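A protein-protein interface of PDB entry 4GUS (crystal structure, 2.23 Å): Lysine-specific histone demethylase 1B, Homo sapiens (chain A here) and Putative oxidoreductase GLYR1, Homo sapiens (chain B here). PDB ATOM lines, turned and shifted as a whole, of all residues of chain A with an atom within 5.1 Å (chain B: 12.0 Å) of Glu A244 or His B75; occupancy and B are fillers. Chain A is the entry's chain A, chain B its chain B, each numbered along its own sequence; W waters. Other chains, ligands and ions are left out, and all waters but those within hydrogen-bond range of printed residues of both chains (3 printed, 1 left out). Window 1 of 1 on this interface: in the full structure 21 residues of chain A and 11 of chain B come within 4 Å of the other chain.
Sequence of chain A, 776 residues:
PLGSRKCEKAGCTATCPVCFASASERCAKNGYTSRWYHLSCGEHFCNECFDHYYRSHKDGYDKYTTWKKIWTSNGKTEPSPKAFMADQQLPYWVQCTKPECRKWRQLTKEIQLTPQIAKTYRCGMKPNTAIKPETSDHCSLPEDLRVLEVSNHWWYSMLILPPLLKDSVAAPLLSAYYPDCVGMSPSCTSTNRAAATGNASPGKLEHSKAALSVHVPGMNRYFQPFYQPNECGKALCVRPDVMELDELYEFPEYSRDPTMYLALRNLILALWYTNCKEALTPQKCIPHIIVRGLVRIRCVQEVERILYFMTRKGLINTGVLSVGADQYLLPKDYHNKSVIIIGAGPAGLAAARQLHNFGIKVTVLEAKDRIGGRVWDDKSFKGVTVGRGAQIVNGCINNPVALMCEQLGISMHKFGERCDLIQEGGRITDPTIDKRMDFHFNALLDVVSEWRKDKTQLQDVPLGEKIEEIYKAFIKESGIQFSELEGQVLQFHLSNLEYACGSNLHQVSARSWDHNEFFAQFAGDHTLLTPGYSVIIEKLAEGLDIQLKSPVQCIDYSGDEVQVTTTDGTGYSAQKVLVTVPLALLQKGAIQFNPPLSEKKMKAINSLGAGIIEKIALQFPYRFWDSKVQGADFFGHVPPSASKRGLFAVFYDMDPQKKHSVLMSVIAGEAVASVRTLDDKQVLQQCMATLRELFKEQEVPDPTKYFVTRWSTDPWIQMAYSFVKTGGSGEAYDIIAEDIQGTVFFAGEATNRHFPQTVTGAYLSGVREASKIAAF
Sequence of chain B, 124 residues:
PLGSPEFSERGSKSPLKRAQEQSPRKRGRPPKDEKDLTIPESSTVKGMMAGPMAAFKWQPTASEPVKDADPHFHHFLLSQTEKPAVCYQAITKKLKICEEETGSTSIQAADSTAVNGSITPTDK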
ATOM      1  N   LEU A 236      10.414  17.752   9.463  1.00  0.00           N
ATOM      2  CA  LEU A 236       8.971  18.027   9.395  1.00  0.00           C
ATOM      3  C   LEU A 236       8.509  19.071  10.432  1.00  0.00           C
ATOM      4  O   LEU A 236       7.501  18.915  11.108  1.00  0.00           O
ATOM      5  CB  LEU A 236       8.149  16.736   9.454  1.00  0.00           C
ATOM      6  CG  LEU A 236       8.496  15.611   8.451  1.00  0.00           C
ATOM      7  CD1 LEU A 236       7.378  14.557   8.393  1.00  0.00           C
ATOM      8  CD2 LEU A 236       8.868  16.102   7.031  1.00  0.00           C
ATOM      9  N   CYS A 237       9.269  20.145  10.545  1.00  0.00           N
ATOM     10  CA  CYS A 237       8.900  21.204  11.462  1.00  0.00           C
ATOM     11  C   CYS A 237       8.625  22.481  10.661  1.00  0.00           C
ATOM     12  O   CYS A 237       9.385  22.799   9.747  1.00  0.00           O
ATOM     13  CB  CYS A 237      10.035  21.428  12.463  1.00  0.00           C
ATOM     14  SG  CYS A 237       9.523  22.128  14.032  1.00  0.00           S
ATOM     15  N   VAL A 238       7.544  23.195  10.987  1.00  0.00           N
ATOM     16  CA  VAL A 238       7.274  24.505  10.370  1.00  0.00           C
ATOM     17  C   VAL A 238       7.532  25.686  11.315  1.00  0.00           C
ATOM     18  O   VAL A 238       7.277  25.609  12.517  1.00  0.00           O
ATOM     19  CB  VAL A 238       5.805  24.640   9.818  1.00  0.00           C
ATOM     20  CG1 VAL A 238       5.460  23.520   8.854  1.00  0.00           C
ATOM     21  CG2 VAL A 238       4.778  24.728  10.941  1.00  0.00           C
ATOM     22  N   ARG A 239       8.030  26.787  10.769  1.00  0.00           N
ATOM     23  CA  ARG A 239       8.033  28.050  11.512  1.00  0.00           C
ATOM     24  C   ARG A 239       6.610  28.582  11.676  1.00  0.00           C
ATOM     25  O   ARG A 239       5.855  28.706  10.708  1.00  0.00           O
ATOM     26  CB  ARG A 239       8.884  29.094  10.817  1.00  0.00           C
ATOM     27  CG  ARG A 239      10.353  28.875  10.998  1.00  0.00           C
ATOM     28  CD  ARG A 239      10.982  30.151  11.498  1.00  0.00           C
ATOM     29  NE  ARG A 239      11.829  30.763  10.483  1.00  0.00           N
ATOM     30  CZ  ARG A 239      12.472  31.912  10.657  1.00  0.00           C
ATOM     31  NH1 ARG A 239      12.342  32.569  11.809  1.00  0.00           N
ATOM     32  NH2 ARG A 239      13.232  32.402   9.679  1.00  0.00           N
ATOM     33  N   VAL A 242       6.533  32.160   9.930  1.00  0.00           N
ATOM     34  CA  VAL A 242       7.052  32.344   8.577  1.00  0.00           C
ATOM     35  C   VAL A 242       6.402  31.324   7.652  1.00  0.00           C
ATOM     36  O   VAL A 242       6.212  30.157   8.022  1.00  0.00           O
ATOM     37  CB  VAL A 242       8.603  32.214   8.511  1.00  0.00           C
ATOM     38  CG1 VAL A 242       9.103  32.414   7.088  1.00  0.00           C
ATOM     39  CG2 VAL A 242       9.277  33.217   9.425  1.00  0.00           C
ATOM     40  N   MET A 243       6.046  31.763   6.450  1.00  0.00           N
ATOM     41  CA  MET A 243       5.408  30.878   5.492  1.00  0.00           C
ATOM     42  C   MET A 243       6.470  30.079   4.774  1.00  0.00           C
ATOM     43  O   MET A 243       7.519  30.618   4.411  1.00  0.00           O
ATOM     44  CB  MET A 243       4.574  31.673   4.489  1.00  0.00           C
ATOM     45  CG  MET A 243       3.297  32.256   5.070  1.00  0.00           C
ATOM     46  SD  MET A 243       2.411  33.295   3.866  1.00  0.00           S
ATOM     47  CE  MET A 243       1.450  32.066   2.972  1.00  0.00           C
ATOM     48  N   GLU A 244       6.209  28.787   4.596  1.00  0.00           N
ATOM     49  CA  GLU A 244       7.108  27.921   3.836  1.00  0.00           C
ATOM     50  C   GLU A 244       7.018  28.265   2.352  1.00  0.00           C
ATOM     51  O   GLU A 244       6.060  28.903   1.924  1.00  0.00           O
ATOM     52  CB  GLU A 244       6.718  26.459   4.035  1.00  0.00           C
ATOM     53  CG  GLU A 244       6.745  25.991   5.477  1.00  0.00           C
ATOM     54  CD  GLU A 244       8.149  25.727   5.983  1.00  0.00           C
ATOM     55  OE1 GLU A 244       8.398  25.972   7.184  1.00  0.00           O
ATOM     56  OE2 GLU A 244       9.007  25.271   5.190  1.00  0.00           O
ATOM     57  N   LEU A 245       7.990  27.805   1.573  1.00  0.00           N
ATOM     58  CA  LEU A 245       8.060  28.102   0.137  1.00  0.00           C
ATOM     59  C   LEU A 245       6.791  27.751  -0.621  1.00  0.00           C
ATOM     60  O   LEU A 245       6.274  28.561  -1.392  1.00  0.00           O
ATOM     61  CB  LEU A 245       9.259  27.404  -0.511  1.00  0.00           C
ATOM     62  CG  LEU A 245      10.624  27.842   0.024  1.00  0.00           C
ATOM     63  CD1 LEU A 245      11.789  27.080  -0.657  1.00  0.00           C
ATOM     64  CD2 LEU A 245      10.796  29.363  -0.103  1.00  0.00           C
ATOM     65  N   ASP A 246       6.275  26.553  -0.393  1.00  0.00           N
ATOM     66  CA  ASP A 246       5.094  26.112  -1.124  1.00  0.00           C
ATOM     67  C   ASP A 246       3.864  26.843  -0.638  1.00  0.00           C
ATOM     68  O   ASP A 246       2.864  26.886  -1.336  1.00  0.00           O
ATOM     69  CB  ASP A 246       4.854  24.607  -0.959  1.00  0.00           C
ATOM     70  CG  ASP A 246       5.955  23.765  -1.570  1.00  0.00           C
ATOM     71  OD1 ASP A 246       6.936  24.338  -2.084  1.00  0.00           O
ATOM     72  OD2 ASP A 246       5.839  22.525  -1.522  1.00  0.00           O
ATOM     73  N   GLU A 247       3.905  27.356   0.586  1.00  0.00           N
ATOM     74  CA  GLU A 247       2.771  28.133   1.068  1.00  0.00           C
ATOM     75  C   GLU A 247       2.747  29.487   0.345  1.00  0.00           C
ATOM     76  O   GLU A 247       1.696  29.951  -0.048  1.00  0.00           O
ATOM     77  CB  GLU A 247       2.818  28.313   2.578  1.00  0.00           C
ATOM     78  CG  GLU A 247       2.597  27.024   3.359  1.00  0.00           C
ATOM     79  CD  GLU A 247       2.773  27.224   4.847  1.00  0.00           C
ATOM     80  OE1 GLU A 247       3.802  27.817   5.241  1.00  0.00           O
ATOM     81  OE2 GLU A 247       1.880  26.796   5.611  1.00  0.00           O
ATOM     82  N   LEU A 248       3.921  30.081   0.145  1.00  0.00           N
ATOM     83  CA  LEU A 248       4.055  31.319  -0.630  1.00  0.00           C
ATOM     84  C   LEU A 248       3.535  31.132  -2.050  1.00  0.00           C
ATOM     85  O   LEU A 248       2.794  31.966  -2.559  1.00  0.00           O
ATOM     86  CB  LEU A 248       5.510  31.787  -0.692  1.00  0.00           C
ATOM     87  CG  LEU A 248       6.005  32.712   0.413  1.00  0.00           C
ATOM     88  CD1 LEU A 248       4.840  33.384   1.159  1.00  0.00           C
ATOM     89  CD2 LEU A 248       6.893  31.972   1.351  1.00  0.00           C
ATOM     90  N   ARG A 265      -3.188  28.229   9.542  1.00  0.00           N
ATOM     91  CA  ARG A 265      -2.353  27.063   9.311  1.00  0.00           C
ATOM     92  C   ARG A 265      -1.924  26.475  10.671  1.00  0.00           C
ATOM     93  O   ARG A 265      -2.161  25.292  10.932  1.00  0.00           O
ATOM     94  CB  ARG A 265      -1.159  27.421   8.432  1.00  0.00           C
ATOM     95  CG  ARG A 265      -0.126  26.301   8.277  1.00  0.00           C
ATOM     96  CD  ARG A 265       1.087  26.599   9.135  1.00  0.00           C
ATOM     97  NE  ARG A 265       2.187  27.164   8.376  1.00  0.00           N
ATOM     98  CZ  ARG A 265       3.215  27.804   8.919  1.00  0.00           C
ATOM     99  NH1 ARG A 265       3.256  28.014  10.236  1.00  0.00           N
ATOM    100  NH2 ARG A 265       4.192  28.263   8.145  1.00  0.00           N
ATOM    101  N   LEU A 315       0.369  17.043   5.199  1.00  0.00           N
ATOM    102  CA  LEU A 315       0.649  17.504   6.556  1.00  0.00           C
ATOM    103  C   LEU A 315      -0.432  17.059   7.537  1.00  0.00           C
ATOM    104  O   LEU A 315      -0.165  16.904   8.715  1.00  0.00           O
ATOM    105  CB  LEU A 315       0.770  19.029   6.616  1.00  0.00           C
ATOM    106  CG  LEU A 315       1.909  19.856   5.991  1.00  0.00           C
ATOM    107  CD1 LEU A 315       3.041  20.067   6.975  1.00  0.00           C
ATOM    108  CD2 LEU A 315       2.439  19.298   4.675  1.00  0.00           C
ATOM    109  N   ASP B  70      17.351  29.608   3.464  1.00  0.00           N
ATOM    110  CA  ASP B  70      18.182  28.627   4.171  1.00  0.00           C
ATOM    111  C   ASP B  70      17.538  27.245   4.131  1.00  0.00           C
ATOM    112  O   ASP B  70      16.618  26.956   4.910  1.00  0.00           O
ATOM    113  CB  ASP B  70      18.422  29.059   5.625  1.00  0.00           C
ATOM    114  CG  ASP B  70      19.412  28.147   6.365  1.00  0.00           C
ATOM    115  OD1 ASP B  70      20.096  27.310   5.725  1.00  0.00           O
ATOM    116  OD2 ASP B  70      19.513  28.284   7.604  1.00  0.00           O
ATOM    117  N   PRO B  71      18.046  26.370   3.250  1.00  0.00           N
ATOM    118  CA  PRO B  71      17.376  25.101   2.955  1.00  0.00           C
ATOM    119  C   PRO B  71      17.489  24.043   4.063  1.00  0.00           C
ATOM    120  O   PRO B  71      16.830  23.007   3.954  1.00  0.00           O
ATOM    121  CB  PRO B  71      18.088  24.614   1.675  1.00  0.00           C
ATOM    122  CG  PRO B  71      19.235  25.569   1.435  1.00  0.00           C
ATOM    123  CD  PRO B  71      19.392  26.412   2.662  1.00  0.00           C
ATOM    124  N   HIS B  72      18.300  24.286   5.092  1.00  0.00           N
ATOM    125  CA  HIS B  72      18.486  23.293   6.155  1.00  0.00           C
ATOM    126  C   HIS B  72      17.218  23.082   6.966  1.00  0.00           C
ATOM    127  O   HIS B  72      16.911  21.961   7.351  1.00  0.00           O
ATOM    128  CB  HIS B  72      19.620  23.674   7.120  1.00  0.00           C
ATOM    129  CG  HIS B  72      19.732  22.755   8.306  1.00  0.00           C
ATOM    130  ND1 HIS B  72      20.507  21.611   8.298  1.00  0.00           N
ATOM    131  CD2 HIS B  72      19.147  22.800   9.529  1.00  0.00           C
ATOM    132  CE1 HIS B  72      20.407  21.001   9.466  1.00  0.00           C
ATOM    133  NE2 HIS B  72      19.587  21.701  10.233  1.00  0.00           N
ATOM    134  N   PHE B  73      16.482  24.165   7.196  1.00  0.00           N
ATOM    135  CA  PHE B  73      15.374  24.168   8.140  1.00  0.00           C
ATOM    136  C   PHE B  73      14.012  23.813   7.561  1.00  0.00           C
ATOM    137  O   PHE B  73      13.137  23.312   8.291  1.00  0.00           O
ATOM    138  CB  PHE B  73      15.273  25.542   8.802  1.00  0.00           C
ATOM    139  CG  PHE B  73      16.384  25.830   9.777  1.00  0.00           C
ATOM    140  CD1 PHE B  73      16.265  25.467  11.112  1.00  0.00           C
ATOM    141  CD2 PHE B  73      17.546  26.472   9.361  1.00  0.00           C
ATOM    142  CE1 PHE B  73      17.291  25.743  12.023  1.00  0.00           C
ATOM    143  CE2 PHE B  73      18.573  26.751  10.259  1.00  0.00           C
ATOM    144  CZ  PHE B  73      18.446  26.383  11.590  1.00  0.00           C
ATOM    145  N   HIS B  74      13.835  24.089   6.268  1.00  0.00           N
ATOM    146  CA  HIS B  74      12.534  23.988   5.608  1.00  0.00           C
ATOM    147  C   HIS B  74      11.849  22.640   5.795  1.00  0.00           C
ATOM    148  O   HIS B  74      12.501  21.598   5.788  1.00  0.00           O
ATOM    149  CB  HIS B  74      12.667  24.260   4.106  1.00  0.00           C
ATOM    150  CG  HIS B  74      13.231  25.608   3.777  1.00  0.00           C
ATOM    151  ND1 HIS B  74      13.755  25.909   2.535  1.00  0.00           N
ATOM    152  CD2 HIS B  74      13.358  26.732   4.521  1.00  0.00           C
ATOM    153  CE1 HIS B  74      14.181  27.158   2.531  1.00  0.00           C
ATOM    154  NE2 HIS B  74      13.951  27.683   3.723  1.00  0.00           N
ATOM    155  N   HIS B  75      10.531  22.681   5.953  1.00  0.00           N
ATOM    156  CA  HIS B  75       9.717  21.477   5.978  1.00  0.00           C
ATOM    157  C   HIS B  75       9.796  20.756   4.628  1.00  0.00           C
ATOM    158  O   HIS B  75       9.541  21.350   3.580  1.00  0.00           O
ATOM    159  CB  HIS B  75       8.271  21.852   6.292  1.00  0.00           C
ATOM    160  CG  HIS B  75       7.402  20.697   6.695  1.00  0.00           C
ATOM    161  ND1 HIS B  75       7.041  19.694   5.820  1.00  0.00           N
ATOM    162  CD2 HIS B  75       6.786  20.419   7.867  1.00  0.00           C
ATOM    163  CE1 HIS B  75       6.243  18.838   6.443  1.00  0.00           C
ATOM    164  NE2 HIS B  75       6.078  19.253   7.687  1.00  0.00           N
ATOM    165  N   PHE B  76      10.150  19.470   4.671  1.00  0.00           N
ATOM    166  CA  PHE B  76      10.284  18.624   3.480  1.00  0.00           C
ATOM    167  C   PHE B  76       9.052  18.661   2.563  1.00  0.00           C
ATOM    168  O   PHE B  76       9.188  18.732   1.353  1.00  0.00           O
ATOM    169  CB  PHE B  76      10.632  17.178   3.902  1.00  0.00           C
ATOM    170  CG  PHE B  76      10.675  16.181   2.763  1.00  0.00           C
ATOM    171  CD1 PHE B  76      11.797  16.086   1.937  1.00  0.00           C
ATOM    172  CD2 PHE B  76       9.605  15.321   2.536  1.00  0.00           C
ATOM    173  CE1 PHE B  76      11.841  15.162   0.879  1.00  0.00           C
ATOM    174  CE2 PHE B  76       9.644  14.388   1.476  1.00  0.00           C
ATOM    175  CZ  PHE B  76      10.764  14.310   0.656  1.00  0.00           C
ATOM    176  N   LEU B  77       7.857  18.609   3.139  1.00  0.00           N
ATOM    177  CA  LEU B  77       6.644  18.521   2.332  1.00  0.00           C
ATOM    178  C   LEU B  77       6.156  19.864   1.794  1.00  0.00           C
ATOM    179  O   LEU B  77       5.289  19.892   0.920  1.00  0.00           O
ATOM    180  CB  LEU B  77       5.513  17.846   3.111  1.00  0.00           C
ATOM    181  CG  LEU B  77       5.692  16.359   3.452  1.00  0.00           C
ATOM    182  CD1 LEU B  77       4.473  15.867   4.242  1.00  0.00           C
ATOM    183  CD2 LEU B  77       5.931  15.518   2.176  1.00  0.00           C
ATOM    184  N   LEU B  78       6.698  20.961   2.321  1.00  0.00           N
ATOM    185  CA  LEU B  78       6.319  22.316   1.904  1.00  0.00           C
ATOM    186  C   LEU B  78       7.466  23.048   1.204  1.00  0.00           C
ATOM    187  O   LEU B  78       7.532  24.278   1.226  1.00  0.00           O
ATOM    188  CB  LEU B  78       5.872  23.132   3.115  1.00  0.00           C
ATOM    189  CG  LEU B  78       4.625  22.603   3.807  1.00  0.00           C
ATOM    190  CD1 LEU B  78       4.279  23.409   5.071  1.00  0.00           C
ATOM    191  CD2 LEU B  78       3.449  22.542   2.826  1.00  0.00           C
ATOM    192  N   SER B  79       8.376  22.291   0.597  1.00  0.00           N
ATOM    193  CA  SER B  79       9.493  22.871  -0.128  1.00  0.00           C
ATOM    194  C   SER B  79       9.680  22.141  -1.440  1.00  0.00           C
ATOM    195  O   SER B  79      10.755  22.169  -2.026  1.00  0.00           O
ATOM    196  CB  SER B  79      10.771  22.787   0.699  1.00  0.00           C
ATOM    197  OG  SER B  79      10.502  23.141   2.043  1.00  0.00           O
ATOM    198  N   GLN B  80       8.611  21.509  -1.906  1.00  0.00           N
ATOM    199  CA  GLN B  80       8.612  20.832  -3.203  1.00  0.00           C
ATOM    200  C   GLN B  80       8.448  21.799  -4.372  1.00  0.00           C
ATOM    201  O   GLN B  80       8.279  21.367  -5.512  1.00  0.00           O
ATOM    202  CB  GLN B  80       7.507  19.775  -3.228  1.00  0.00           C
ATOM    203  CG  GLN B  80       7.722  18.696  -2.156  1.00  0.00           C
ATOM    204  CD  GLN B  80       9.020  17.948  -2.371  1.00  0.00           C
ATOM    205  OE1 GLN B  80       9.372  17.632  -3.506  1.00  0.00           O
ATOM    206  NE2 GLN B  80       9.748  17.673  -1.286  1.00  0.00           N
ATOM    207  N   THR B  81       8.526  23.094  -4.061  1.00  0.00           N
ATOM    208  CA  THR B  81       8.237  24.229  -4.964  1.00  0.00           C
ATOM    209  C   THR B  81       6.948  24.101  -5.785  1.00  0.00           C
ATOM    210  O   THR B  81       5.893  24.629  -5.393  1.00  0.00           O
ATOM    211  CB  THR B  81       9.444  24.640  -5.854  1.00  0.00           C
ATOM    212  OG1 THR B  81       9.554  23.748  -6.966  1.00  0.00           O
ATOM    213  CG2 THR B  81      10.747  24.638  -5.051  1.00  0.00           C
HETATM  214  O   HOH W   1      11.714  18.739   7.036  1.00  0.00           O
HETATM  215  O   HOH W   2      11.659  20.708   8.910  1.00  0.00           O
HETATM  216  O   HOH W   3      10.059  26.010   3.120  1.00  0.00           O
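Among the printed residues, merely in contact across the chains: Leu A315 with His B75 (3.2 Å), Leu A236 with His B75 (3.4 Å), Val A238 with His B75 (3.5 Å), Glu A244 with Leu B78 (3.6 Å), Leu A245 with Leu B78 (3.6 Å), Asp A246 with Leu B77 (3.6 Å), Cys A237 with His B75 (3.7 Å), Leu A315 with Leu B77 (3.7 Å), Leu A236 with Phe B76 (3.7 Å), Glu A244 with His B74 (3.8 Å), Leu A315 with Leu B78 (3.9 Å), Leu A245 with His B74 (3.9 Å) and Val A238 with Leu B78 (3.96 Å).
The backbone NH of Asp A246 lies within hydrogen-bond range of the backbone carbonyl oxygen of Leu B78.
OD2 of Asp A246 is in hydrogen-bond range of N of Gln B80 (3.0 Å).
OD1 of Asp A246 sits at hydrogen-bond distance from N of Thr B81, at 2.8 Å.
The backbone NH (N) of Ser B79 lies within hydrogen-bond range of the side-chain carboxylate (OD2) of Asp A246 (3.3 Å).
OE2 of Glu A244 sits at hydrogen-bond distance from N of His B75, 3.1 Å away.
Of chain B, only His B74, His B75 and Leu B78 come within 4 Å of Glu A244.
Of chain A, only Leu A236, Cys A237, Val A238, Glu A244 and Leu A315 come within 4 Å of His B75.
Val A238 touches just these residues of chain B: His B75 and Leu B78.
No residue of chain B comes within 4 Å of Val A242.
No residue of chain B comes within 4 Å of Met A243.
Glu A247 touches none of the printed residues of chain B.
Leu A248 touches none of the printed residues of chain B.
Leu A315 touches just these residues of chain B: His B75 (3.2 Å), Leu B77 (3.7 Å) and Leu B78 (3.9 Å).
Printed residues of chain A within 4 Å of Phe B76: Leu A236.
Printed residues of chain A within 4 Å of Gln B80: Asp A246.
Printed residues of chain A within 4 Å of Leu B77: Asp A246 (3.6 Å) and Leu A315 (3.7 Å).
Of the printed residues of chain A, Ser B79 touches Asp A246.
Printed residues of chain A within 4 Å of His B74: Glu A244 and Leu A245.
Arg A239 touches none of the printed residues of chain B.
Phe B73 touches none of the printed residues of chain A.
The nearest residue of chain B that does not touch Glu A244 is Ser B79 (4.1 Å).
The backbone NH (N) of Glu A244 lies within hydrogen-bond range of the side-chain carboxylate (OE1) of Glu A247 (2.7 Å).
O of His B75 is in hydrogen-bond range of OG of Ser B79, at 2.5 Å.
The backbone carbonyl oxygen (O) of Asp B70 sits at hydrogen-bond distance from a ring nitrogen (NE2) of His B74.
ND1 of His B75 lies within hydrogen-bond range of N of Leu B77 (3.0 Å).
The backbone carbonyl oxygen (O) of Phe B76 lies within hydrogen-bond range of the side-chain amide nitrogen (NE2) of Gln B80, at 2.9 Å.
Water W3 lies within hydrogen-bond range of the side-chain carboxylate of Glu A244 (2.4 Å), the side-chain hydroxyl of Ser B79 (3.1 Å) and the backbone NH of Leu A245 (3.1 Å).
Water W1 lies within hydrogen-bond range of the backbone NH of Leu A236 (2.9 Å), the backbone NH of Phe B76 (2.9 Å) and the backbone carbonyl oxygen of His B74 (3.2 Å).
Water W2 lies within hydrogen-bond range of the backbone NH (N) of Cys A237 (2.9 Å), the backbone carbonyl oxygen (O) of Phe B73 (3.1 Å), the backbone NH (N) of Leu A236 (3.3 Å) and the backbone carbonyl oxygen (O) of His B74 (3.4 Å).
Hydrophobic or aromatic side chains of chain B within 4 Å of the printed part of chain A: His B74, His B75, Phe B76, Leu B77 and Leu B78.
Hydrophobic or aromatic side chains of chain A within 4 Å of the printed part of chain B: Leu A236, Val A238, Leu A245 and Leu A315.
Among the printed residues, 18 pairs touch across the chains.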
